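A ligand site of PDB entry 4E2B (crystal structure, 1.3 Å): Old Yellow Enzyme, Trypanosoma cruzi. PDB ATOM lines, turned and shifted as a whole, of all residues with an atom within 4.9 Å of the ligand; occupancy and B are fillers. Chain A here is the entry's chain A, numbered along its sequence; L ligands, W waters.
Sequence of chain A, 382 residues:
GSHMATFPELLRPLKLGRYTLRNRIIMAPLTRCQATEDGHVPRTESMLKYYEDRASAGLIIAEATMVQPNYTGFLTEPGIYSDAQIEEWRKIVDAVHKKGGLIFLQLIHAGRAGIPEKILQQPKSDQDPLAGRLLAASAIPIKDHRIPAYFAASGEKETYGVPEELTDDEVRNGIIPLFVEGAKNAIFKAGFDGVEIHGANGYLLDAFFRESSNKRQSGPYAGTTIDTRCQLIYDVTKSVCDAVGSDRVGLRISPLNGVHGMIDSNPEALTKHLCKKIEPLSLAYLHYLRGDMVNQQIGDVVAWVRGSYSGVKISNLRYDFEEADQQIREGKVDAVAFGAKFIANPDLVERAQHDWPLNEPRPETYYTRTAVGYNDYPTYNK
The side-chain amide nitrogen (ND2) of Asn 316 is in hydrogen-bond range of an oxygen (O4) of the ligand, 2.7 Å away.
The backbone NH (N) of Thr 31 is in hydrogen-bond range of a nitrogen (N3) of the ligand (2.7 Å).
O2 of the ligand sits at hydrogen-bond distance from OG1 of Thr 31 (2.7 Å).
An oxygen (O1) of the ligand lies within hydrogen-bond range of the guanidinium group (NH2) of Arg 252.
O of Pro 29 lies within hydrogen-bond range of O3 of the ligand, 2.8 Å away.
An oxygen (O7) of the ligand is in hydrogen-bond range of the backbone NH (N) of Arg 318, 2.8 Å away.
N2 of the ligand sits at hydrogen-bond distance from OE1 of Gln 106, 2.8 Å away.
An oxygen (O9) of the ligand sits at hydrogen-bond distance from the backbone NH (N) of Gly 339, 2.8 Å away.
The backbone NH of Ala 340 sits at hydrogen-bond distance from an oxygen (O8) of the ligand (2.8 Å).
An oxygen (O1) of the ligand sits at hydrogen-bond distance from a ring nitrogen (NE2) of His 198.
O2 of the ligand sits close to N of Ala 64 (3.3 Å).
The side-chain amide nitrogen (ND2) of Asn 316 sits close to the guanidinium group (NH1) of Arg 252.
The side-chain amide oxygen (OD1) of Asn 316 lies close to the backbone carbonyl oxygen (O) of Ala 337, 2.9 Å away.
The side-chain amide oxygen (OE1) of Gln 106 sits close to the backbone NH (N) of Ala 64, 3.4 Å away.
N of Ala 28 is in hydrogen-bond range of O of Phe 338 (3.0 Å).
NE of Arg 32 lies within hydrogen-bond range of O of Tyr 366 (3.0 Å).
Ala 28 touches the ligand (CB to O3, 3.4 Å).
Leu 30 touches the ligand.
OD1 of Asn 201 touches N1 of the ligand, at 3.6 Å.
Leu 289 touches the ligand.
CD1 of Leu 317 touches C17 of the ligand (3.7 Å).
Phe 338 touches the ligand.
Tyr 366 touches the ligand (CD2 to C7, 3.7 Å).
Tyr 367 touches the ligand.
Within 4 Å of the ligand: Ala 28, Pro 29, Leu 30, Thr 31, Ala 64, Gln 106, His 198, Asn 201, Arg 252, Leu 289, Asn 316, Leu 317, Arg 318, Phe 338, Gly 339, Ala 340, Tyr 366 and Tyr 367.
The nearest printed residue that does not touch the ligand is Ile 343 (4.1 Å).
Water W8 lies within hydrogen-bond range of an oxygen (O9) of the ligand (2.8 Å), the backbone NH of Gly 339 (3.5 Å) and the backbone NH of Ala 340 (3.5 Å).
Water W5 bridges O2 of the ligand (3.1 Å) and NE2 of His 198 (3.2 Å).
Water W7 lies within hydrogen-bond range of O5 of the ligand (3.1 Å) and SD of Met 293 (3.6 Å).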
ATOM      1  N   ALA A  28     -17.279   6.928  12.588  1.00  0.00           N
ATOM      2  CA  ALA A  28     -16.904   8.093  13.370  1.00  0.00           C
ATOM      3  C   ALA A  28     -17.430   9.373  12.728  1.00  0.00           C
ATOM      4  O   ALA A  28     -17.606   9.416  11.502  1.00  0.00           O
ATOM      5  CB  ALA A  28     -15.385   8.155  13.519  1.00  0.00           C
ATOM      6  N   PRO A  29     -17.667  10.422  13.528  1.00  0.00           N
ATOM      7  CA  PRO A  29     -18.073  11.712  12.976  1.00  0.00           C
ATOM      8  C   PRO A  29     -16.954  12.297  12.111  1.00  0.00           C
ATOM      9  O   PRO A  29     -15.795  12.344  12.550  1.00  0.00           O
ATOM     10  CB  PRO A  29     -18.338  12.568  14.211  1.00  0.00           C
ATOM     11  CG  PRO A  29     -17.514  11.951  15.289  1.00  0.00           C
ATOM     12  CD  PRO A  29     -17.496  10.482  14.996  1.00  0.00           C
ATOM     13  N   LEU A  30     -17.304  12.726  10.895  1.00  0.00           N
ATOM     14  CA  LEU A  30     -16.323  13.231   9.938  1.00  0.00           C
ATOM     15  C   LEU A  30     -16.836  14.488   9.236  1.00  0.00           C
ATOM     16  O   LEU A  30     -17.719  14.402   8.374  1.00  0.00           O
ATOM     17  CB  LEU A  30     -15.988  12.151   8.899  1.00  0.00           C
ATOM     18  CG  LEU A  30     -15.381  10.857   9.424  1.00  0.00           C
ATOM     19  CD1 LEU A  30     -15.744   9.671   8.544  1.00  0.00           C
ATOM     20  CD2 LEU A  30     -13.864  10.997   9.572  1.00  0.00           C
ATOM     21  N   THR A  31     -16.284  15.637   9.606  1.00  0.00           N
ATOM     22  CA  THR A  31     -16.555  16.917   8.942  1.00  0.00           C
ATOM     23  C   THR A  31     -16.120  16.835   7.488  1.00  0.00           C
ATOM     24  O   THR A  31     -14.942  16.595   7.204  1.00  0.00           O
ATOM     25  CB  THR A  31     -15.785  18.044   9.659  1.00  0.00           C
ATOM     26  OG1 THR A  31     -16.354  18.252  10.954  1.00  0.00           O
ATOM     27  CG2 THR A  31     -15.841  19.345   8.895  1.00  0.00           C
ATOM     28  N   ARG A  32     -17.081  17.019   6.576  1.00  0.00           N
ATOM     29  CA  ARG A  32     -16.804  16.993   5.131  1.00  0.00           C
ATOM     30  C   ARG A  32     -17.160  18.301   4.414  1.00  0.00           C
ATOM     31  O   ARG A  32     -16.888  18.430   3.228  1.00  0.00           O
ATOM     32  CB  ARG A  32     -17.497  15.795   4.458  1.00  0.00           C
ATOM     33  CG  ARG A  32     -17.275  14.434   5.130  1.00  0.00           C
ATOM     34  CD  ARG A  32     -15.810  14.059   5.296  1.00  0.00           C
ATOM     35  NE  ARG A  32     -15.073  14.077   4.025  1.00  0.00           N
ATOM     36  CZ  ARG A  32     -15.095  13.113   3.120  1.00  0.00           C
ATOM     37  NH1 ARG A  32     -14.409  13.240   2.000  1.00  0.00           N
ATOM     38  NH2 ARG A  32     -15.807  12.000   3.332  1.00  0.00           N
ATOM     39  N   GLU A  63     -21.457  13.944  11.160  1.00  0.00           N
ATOM     40  CA  GLU A  63     -20.459  14.997  11.368  1.00  0.00           C
ATOM     41  C   GLU A  63     -20.875  16.094  12.333  1.00  0.00           C
ATOM     42  O   GLU A  63     -22.063  16.382  12.488  1.00  0.00           O
ATOM     43  CB  GLU A  63     -20.119  15.644  10.034  1.00  0.00           C
ATOM     44  CG  GLU A  63     -21.279  16.329   9.333  1.00  0.00           C
ATOM     45  CD  GLU A  63     -21.117  16.234   7.840  1.00  0.00           C
ATOM     46  OE1 GLU A  63     -20.186  16.873   7.291  1.00  0.00           O
ATOM     47  OE2 GLU A  63     -21.912  15.493   7.222  1.00  0.00           O
ATOM     48  N   ALA A  64     -19.878  16.732  12.933  1.00  0.00           N
ATOM     49  CA  ALA A  64     -20.072  17.874  13.815  1.00  0.00           C
ATOM     50  C   ALA A  64     -21.045  18.878  13.212  1.00  0.00           C
ATOM     51  O   ALA A  64     -20.839  19.378  12.094  1.00  0.00           O
ATOM     52  CB  ALA A  64     -18.736  18.535  14.123  1.00  0.00           C
ATOM     53  N   GLN A 106     -23.726  14.438  15.826  1.00  0.00           N
ATOM     54  CA  GLN A 106     -22.772  15.088  16.719  1.00  0.00           C
ATOM     55  C   GLN A 106     -23.052  16.592  16.803  1.00  0.00           C
ATOM     56  O   GLN A 106     -23.169  17.262  15.767  1.00  0.00           O
ATOM     57  CB  GLN A 106     -21.331  14.832  16.295  1.00  0.00           C
ATOM     58  CG  GLN A 106     -20.328  15.255  17.345  1.00  0.00           C
ATOM     59  CD  GLN A 106     -18.893  15.152  16.877  1.00  0.00           C
ATOM     60  OE1 GLN A 106     -18.510  15.745  15.869  1.00  0.00           O
ATOM     61  NE2 GLN A 106     -18.082  14.406  17.618  1.00  0.00           N
ATOM     62  N   HIS A 198     -20.159  16.774  21.514  1.00  0.00           N
ATOM     63  CA  HIS A 198     -18.763  16.904  21.114  1.00  0.00           C
ATOM     64  C   HIS A 198     -17.922  17.504  22.221  1.00  0.00           C
ATOM     65  O   HIS A 198     -17.790  18.736  22.319  1.00  0.00           O
ATOM     66  CB  HIS A 198     -18.624  17.733  19.847  1.00  0.00           C
ATOM     67  CG  HIS A 198     -17.313  17.528  19.123  1.00  0.00           C
ATOM     68  ND1 HIS A 198     -16.193  17.116  19.754  1.00  0.00           N
ATOM     69  CD2 HIS A 198     -16.970  17.718  17.791  1.00  0.00           C
ATOM     70  CE1 HIS A 198     -15.192  17.018  18.848  1.00  0.00           C
ATOM     71  NE2 HIS A 198     -15.665  17.403  17.657  1.00  0.00           N
ATOM     72  N   ASN A 201     -11.370  17.191  20.949  1.00  0.00           N
ATOM     73  CA  ASN A 201     -10.629  17.801  19.836  1.00  0.00           C
ATOM     74  C   ASN A 201     -10.470  19.325  19.881  1.00  0.00           C
ATOM     75  O   ASN A 201     -10.302  19.965  18.833  1.00  0.00           O
ATOM     76  CB  ASN A 201     -11.189  17.321  18.488  1.00  0.00           C
ATOM     77  CG  ASN A 201     -11.180  15.800  18.335  1.00  0.00           C
ATOM     78  OD1 ASN A 201     -11.956  15.218  17.570  1.00  0.00           O
ATOM     79  ND2 ASN A 201     -10.298  15.135  19.077  1.00  0.00           N
ATOM     80  N   ARG A 252     -18.563  12.284  23.349  1.00  0.00           N
ATOM     81  CA  ARG A 252     -17.221  12.025  22.836  1.00  0.00           C
ATOM     82  C   ARG A 252     -16.169  12.866  23.554  1.00  0.00           C
ATOM     83  O   ARG A 252     -16.357  14.077  23.746  1.00  0.00           O
ATOM     84  CB  ARG A 252     -17.130  12.262  21.328  1.00  0.00           C
ATOM     85  CG  ARG A 252     -15.908  11.601  20.729  1.00  0.00           C
ATOM     86  CD  ARG A 252     -15.736  11.862  19.240  1.00  0.00           C
ATOM     87  NE  ARG A 252     -15.131  10.693  18.613  1.00  0.00           N
ATOM     88  CZ  ARG A 252     -14.467  10.697  17.460  1.00  0.00           C
ATOM     89  NH1 ARG A 252     -13.997   9.556  16.973  1.00  0.00           N
ATOM     90  NH2 ARG A 252     -14.254  11.819  16.800  1.00  0.00           N
ATOM     91  N   LEU A 289     -11.387   9.032  21.810  1.00  0.00           N
ATOM     92  CA  LEU A 289     -10.122   8.805  21.116  1.00  0.00           C
ATOM     93  C   LEU A 289      -9.124   8.230  22.132  1.00  0.00           C
ATOM     94  O   LEU A 289      -8.939   8.798  23.217  1.00  0.00           O
ATOM     95  CB  LEU A 289      -9.575  10.094  20.504  1.00  0.00           C
ATOM     96  CG  LEU A 289     -10.104  10.517  19.133  1.00  0.00           C
ATOM     97  CD1 LEU A 289     -11.536  10.990  19.198  1.00  0.00           C
ATOM     98  CD2 LEU A 289      -9.206  11.591  18.554  1.00  0.00           C
ATOM     99  N   MET A 293      -3.405  12.270  17.947  1.00  0.00           N
ATOM    100  CA  MET A 293      -3.163  12.363  16.515  1.00  0.00           C
ATOM    101  C   MET A 293      -1.779  12.972  16.223  1.00  0.00           C
ATOM    102  O   MET A 293      -1.233  12.778  15.140  1.00  0.00           O
ATOM    103  CB  MET A 293      -4.298  13.109  15.808  1.00  0.00           C
ATOM    104  CG  MET A 293      -5.658  12.433  15.989  1.00  0.00           C
ATOM    105  SD  MET A 293      -7.001  13.022  14.930  1.00  0.00           S
ATOM    106  CE  MET A 293      -7.240  14.685  15.554  1.00  0.00           C
ATOM    107  N   ASN A 316     -11.795   4.718  19.522  1.00  0.00           N
ATOM    108  CA  ASN A 316     -11.417   5.200  18.201  1.00  0.00           C
ATOM    109  C   ASN A 316      -9.945   5.583  18.204  1.00  0.00           C
ATOM    110  O   ASN A 316      -9.398   5.967  19.241  1.00  0.00           O
ATOM    111  CB  ASN A 316     -12.252   6.430  17.823  1.00  0.00           C
ATOM    112  CG  ASN A 316     -11.733   7.127  16.587  1.00  0.00           C
ATOM    113  OD1 ASN A 316     -12.006   6.731  15.450  1.00  0.00           O
ATOM    114  ND2 ASN A 316     -10.945   8.167  16.798  1.00  0.00           N
ATOM    115  N   LEU A 317      -9.345   5.459  17.024  1.00  0.00           N
ATOM    116  CA  LEU A 317      -8.045   6.035  16.590  1.00  0.00           C
ATOM    117  C   LEU A 317      -7.091   4.925  16.182  1.00  0.00           C
ATOM    118  O   LEU A 317      -6.622   4.146  17.024  1.00  0.00           O
ATOM    119  CB  LEU A 317      -7.379   6.979  17.607  1.00  0.00           C
ATOM    120  CG  LEU A 317      -6.080   7.618  17.108  1.00  0.00           C
ATOM    121  CD1 LEU A 317      -6.293   8.549  15.924  1.00  0.00           C
ATOM    122  CD2 LEU A 317      -5.419   8.373  18.258  1.00  0.00           C
ATOM    123  N   ARG A 318      -6.843   4.854  14.876  1.00  0.00           N
ATOM    124  CA  ARG A 318      -5.855   3.933  14.290  1.00  0.00           C
ATOM    125  C   ARG A 318      -6.147   2.443  14.546  1.00  0.00           C
ATOM    126  O   ARG A 318      -5.222   1.636  14.706  1.00  0.00           O
ATOM    127  CB  ARG A 318      -4.431   4.317  14.721  1.00  0.00           C
ATOM    128  CG  ARG A 318      -3.997   5.705  14.264  1.00  0.00           C
ATOM    129  CD  ARG A 318      -2.539   6.002  14.590  1.00  0.00           C
ATOM    130  NE  ARG A 318      -2.305   6.307  16.000  1.00  0.00           N
ATOM    131  CZ  ARG A 318      -2.125   7.523  16.507  1.00  0.00           C
ATOM    132  NH1 ARG A 318      -1.908   7.672  17.804  1.00  0.00           N
ATOM    133  NH2 ARG A 318      -2.153   8.589  15.714  1.00  0.00           N
ATOM    134  N   TYR A 319      -7.425   2.075  14.597  1.00  0.00           N
ATOM    135  CA  TYR A 319      -7.801   0.661  14.670  1.00  0.00           C
ATOM    136  C   TYR A 319      -7.886   0.061  13.279  1.00  0.00           C
ATOM    137  O   TYR A 319      -8.393   0.710  12.350  1.00  0.00           O
ATOM    138  CB  TYR A 319      -9.164   0.482  15.324  1.00  0.00           C
ATOM    139  CG  TYR A 319      -9.169   0.580  16.817  1.00  0.00           C
ATOM    140  CD1 TYR A 319      -9.360   1.805  17.452  1.00  0.00           C
ATOM    141  CD2 TYR A 319      -9.004  -0.554  17.606  1.00  0.00           C
ATOM    142  CE1 TYR A 319      -9.376   1.903  18.829  1.00  0.00           C
ATOM    143  CE2 TYR A 319      -9.012  -0.471  18.983  1.00  0.00           C
ATOM    144  CZ  TYR A 319      -9.201   0.750  19.588  1.00  0.00           C
ATOM    145  OH  TYR A 319      -9.210   0.839  20.957  1.00  0.00           O
ATOM    146  N   ALA A 337     -15.150   2.833  16.543  1.00  0.00           N
ATOM    147  CA  ALA A 337     -15.446   3.769  15.472  1.00  0.00           C
ATOM    148  C   ALA A 337     -14.240   3.934  14.561  1.00  0.00           C
ATOM    149  O   ALA A 337     -13.099   4.050  15.020  1.00  0.00           O
ATOM    150  CB  ALA A 337     -15.886   5.110  16.026  1.00  0.00           C
ATOM    151  N   PHE A 338     -14.521   3.962  13.263  1.00  0.00           N
ATOM    152  CA  PHE A 338     -13.513   4.140  12.230  1.00  0.00           C
ATOM    153  C   PHE A 338     -13.771   5.445  11.493  1.00  0.00           C
ATOM    154  O   PHE A 338     -14.909   5.725  11.110  1.00  0.00           O
ATOM    155  CB  PHE A 338     -13.525   2.966  11.256  1.00  0.00           C
ATOM    156  CG  PHE A 338     -13.288   1.622  11.899  1.00  0.00           C
ATOM    157  CD1 PHE A 338     -12.014   1.084  11.968  1.00  0.00           C
ATOM    158  CD2 PHE A 338     -14.349   0.897  12.429  1.00  0.00           C
ATOM    159  CE1 PHE A 338     -11.790  -0.151  12.559  1.00  0.00           C
ATOM    160  CE2 PHE A 338     -14.142  -0.342  13.033  1.00  0.00           C
ATOM    161  CZ  PHE A 338     -12.861  -0.868  13.083  1.00  0.00           C
ATOM    162  N   GLY A 339     -12.713   6.235  11.306  1.00  0.00           N
ATOM    163  CA  GLY A 339     -12.795   7.506  10.573  1.00  0.00           C
ATOM    164  C   GLY A 339     -12.353   7.381   9.121  1.00  0.00           C
ATOM    165  O   GLY A 339     -13.181   7.208   8.231  1.00  0.00           O
ATOM    166  N   ALA A 340     -11.044   7.432   8.895  1.00  0.00           N
ATOM    167  CA  ALA A 340     -10.511   7.426   7.537  1.00  0.00           C
ATOM    168  C   ALA A 340     -10.985   6.234   6.712  1.00  0.00           C
ATOM    169  O   ALA A 340     -11.258   6.381   5.511  1.00  0.00           O
ATOM    170  CB  ALA A 340      -8.984   7.486   7.566  1.00  0.00           C
ATOM    171  N   ILE A 343     -14.373   7.052   5.292  1.00  0.00           N
ATOM    172  CA  ILE A 343     -14.271   7.990   4.187  1.00  0.00           C
ATOM    173  C   ILE A 343     -14.079   7.203   2.892  1.00  0.00           C
ATOM    174  O   ILE A 343     -14.765   7.442   1.895  1.00  0.00           O
ATOM    175  CB  ILE A 343     -13.100   8.983   4.367  1.00  0.00           C
ATOM    176  CG1 ILE A 343     -13.390   9.927   5.549  1.00  0.00           C
ATOM    177  CG2 ILE A 343     -12.865   9.781   3.084  1.00  0.00           C
ATOM    178  CD1 ILE A 343     -12.282  10.918   5.843  1.00  0.00           C
ATOM    179  N   TYR A 366     -10.181  15.308   1.033  1.00  0.00           N
ATOM    180  CA  TYR A 366     -11.166  15.178   2.129  1.00  0.00           C
ATOM    181  C   TYR A 366     -12.221  16.294   2.129  1.00  0.00           C
ATOM    182  O   TYR A 366     -13.358  16.070   2.560  1.00  0.00           O
ATOM    183  CB  TYR A 366     -10.481  15.136   3.496  1.00  0.00           C
ATOM    184  CG  TYR A 366      -9.838  13.824   3.894  1.00  0.00           C
ATOM    185  CD1 TYR A 366     -10.035  12.644   3.159  1.00  0.00           C
ATOM    186  CD2 TYR A 366      -9.049  13.760   5.043  1.00  0.00           C
ATOM    187  CE1 TYR A 366      -9.432  11.448   3.556  1.00  0.00           C
ATOM    188  CE2 TYR A 366      -8.454  12.580   5.440  1.00  0.00           C
ATOM    189  CZ  TYR A 366      -8.649  11.428   4.701  1.00  0.00           C
ATOM    190  OH  TYR A 366      -8.055  10.247   5.099  1.00  0.00           O
ATOM    191  N   TYR A 367     -11.842  17.486   1.665  1.00  0.00           N
ATOM    192  CA  TYR A 367     -12.677  18.678   1.830  1.00  0.00           C
ATOM    193  C   TYR A 367     -12.904  19.428   0.514  1.00  0.00           C
ATOM    194  O   TYR A 367     -12.820  20.661   0.478  1.00  0.00           O
ATOM    195  CB  TYR A 367     -12.039  19.625   2.855  1.00  0.00           C
ATOM    196  CG  TYR A 367     -11.681  19.027   4.206  1.00  0.00           C
ATOM    197  CD1 TYR A 367     -12.632  18.863   5.214  1.00  0.00           C
ATOM    198  CD2 TYR A 367     -10.355  18.672   4.506  1.00  0.00           C
ATOM    199  CE1 TYR A 367     -12.296  18.344   6.451  1.00  0.00           C
ATOM    200  CE2 TYR A 367     -10.009  18.153   5.741  1.00  0.00           C
ATOM    201  CZ  TYR A 367     -10.981  17.985   6.711  1.00  0.00           C
ATOM    202  OH  TYR A 367     -10.635  17.466   7.946  1.00  0.00           O
HETATM  203  N1  LIG L   1     -14.022  14.033  14.902  1.00  0.00           N
HETATM  204  C1  LIG L   1     -15.112  14.597  15.488  1.00  0.00           C
HETATM  205  O1  LIG L   1     -15.346  14.375  16.695  1.00  0.00           O
HETATM  206  N2  LIG L   1     -15.953  15.370  14.775  1.00  0.00           N
HETATM  207  C2  LIG L   1     -15.764  15.684  13.482  1.00  0.00           C
HETATM  208  O2  LIG L   1     -16.572  16.410  12.868  1.00  0.00           O
HETATM  209  C3  LIG L   1     -14.612  15.108  12.783  1.00  0.00           C
HETATM  210  N3  LIG L   1     -14.350  15.358  11.476  1.00  0.00           N
HETATM  211  C4  LIG L   1     -13.299  14.772  10.867  1.00  0.00           C
HETATM  212  C5  LIG L   1     -13.031  15.002   9.516  1.00  0.00           C
HETATM  213  C6  LIG L   1     -11.943  14.398   8.897  1.00  0.00           C
HETATM  214  C7  LIG L   1     -11.690  14.664   7.436  1.00  0.00           C
HETATM  215  C8  LIG L   1     -11.055  13.508   9.676  1.00  0.00           C
HETATM  216  C9  LIG L   1      -9.855  12.849   9.031  1.00  0.00           C
HETATM  217  C10 LIG L   1     -11.315  13.284  11.016  1.00  0.00           C
HETATM  218  C11 LIG L   1     -12.402  13.881  11.642  1.00  0.00           C
HETATM  219  N4  LIG L   1     -12.657  13.652  13.004  1.00  0.00           N
HETATM  220  C12 LIG L   1     -13.763  14.241  13.600  1.00  0.00           C
HETATM  221  C13 LIG L   1     -11.835  12.732  13.782  1.00  0.00           C
HETATM  222  C14 LIG L   1     -12.402  11.332  13.458  1.00  0.00           C
HETATM  223  O3  LIG L   1     -13.730  11.141  13.977  1.00  0.00           O
HETATM  224  C15 LIG L   1     -11.541  10.214  14.001  1.00  0.00           C
HETATM  225  O4  LIG L   1     -11.435  10.387  15.417  1.00  0.00           O
HETATM  226  C16 LIG L   1     -10.145  10.192  13.359  1.00  0.00           C
HETATM  227  O5  LIG L   1     -10.263  10.134  11.935  1.00  0.00           O
HETATM  228  C17 LIG L   1      -9.297   9.035  13.874  1.00  0.00           C
HETATM  229  O6  LIG L   1      -9.894   7.764  13.580  1.00  0.00           O
HETATM  230  P1  LIG L   1      -9.253   6.838  12.415  1.00  0.00           P
HETATM  231  O7  LIG L   1      -7.848   6.519  12.873  1.00  0.00           O
HETATM  232  O8  LIG L   1      -9.329   7.677  11.157  1.00  0.00           O
HETATM  233  O9  LIG L   1     -10.186   5.657  12.416  1.00  0.00           O
HETATM  234  O   HOH W   1      -7.420   9.392  10.095  1.00  0.00           O
HETATM  235  O   HOH W   2      -9.471  15.118  13.265  1.00  0.00           O
HETATM  236  O   HOH W   3      -6.232   5.254  11.027  1.00  0.00           O
HETATM  237  O   HOH W   4      -5.713   8.159  12.087  1.00  0.00           O
HETATM  238  O   HOH W   5     -15.383  18.535  14.705  1.00  0.00           O
HETATM  239  O   HOH W   6     -10.132   3.979  14.648  1.00  0.00           O
HETATM  240  O   HOH W   7      -7.764  11.941  11.610  1.00  0.00           O
HETATM  241  O   HOH W   8     -10.199   4.247   9.980  1.00  0.00           O
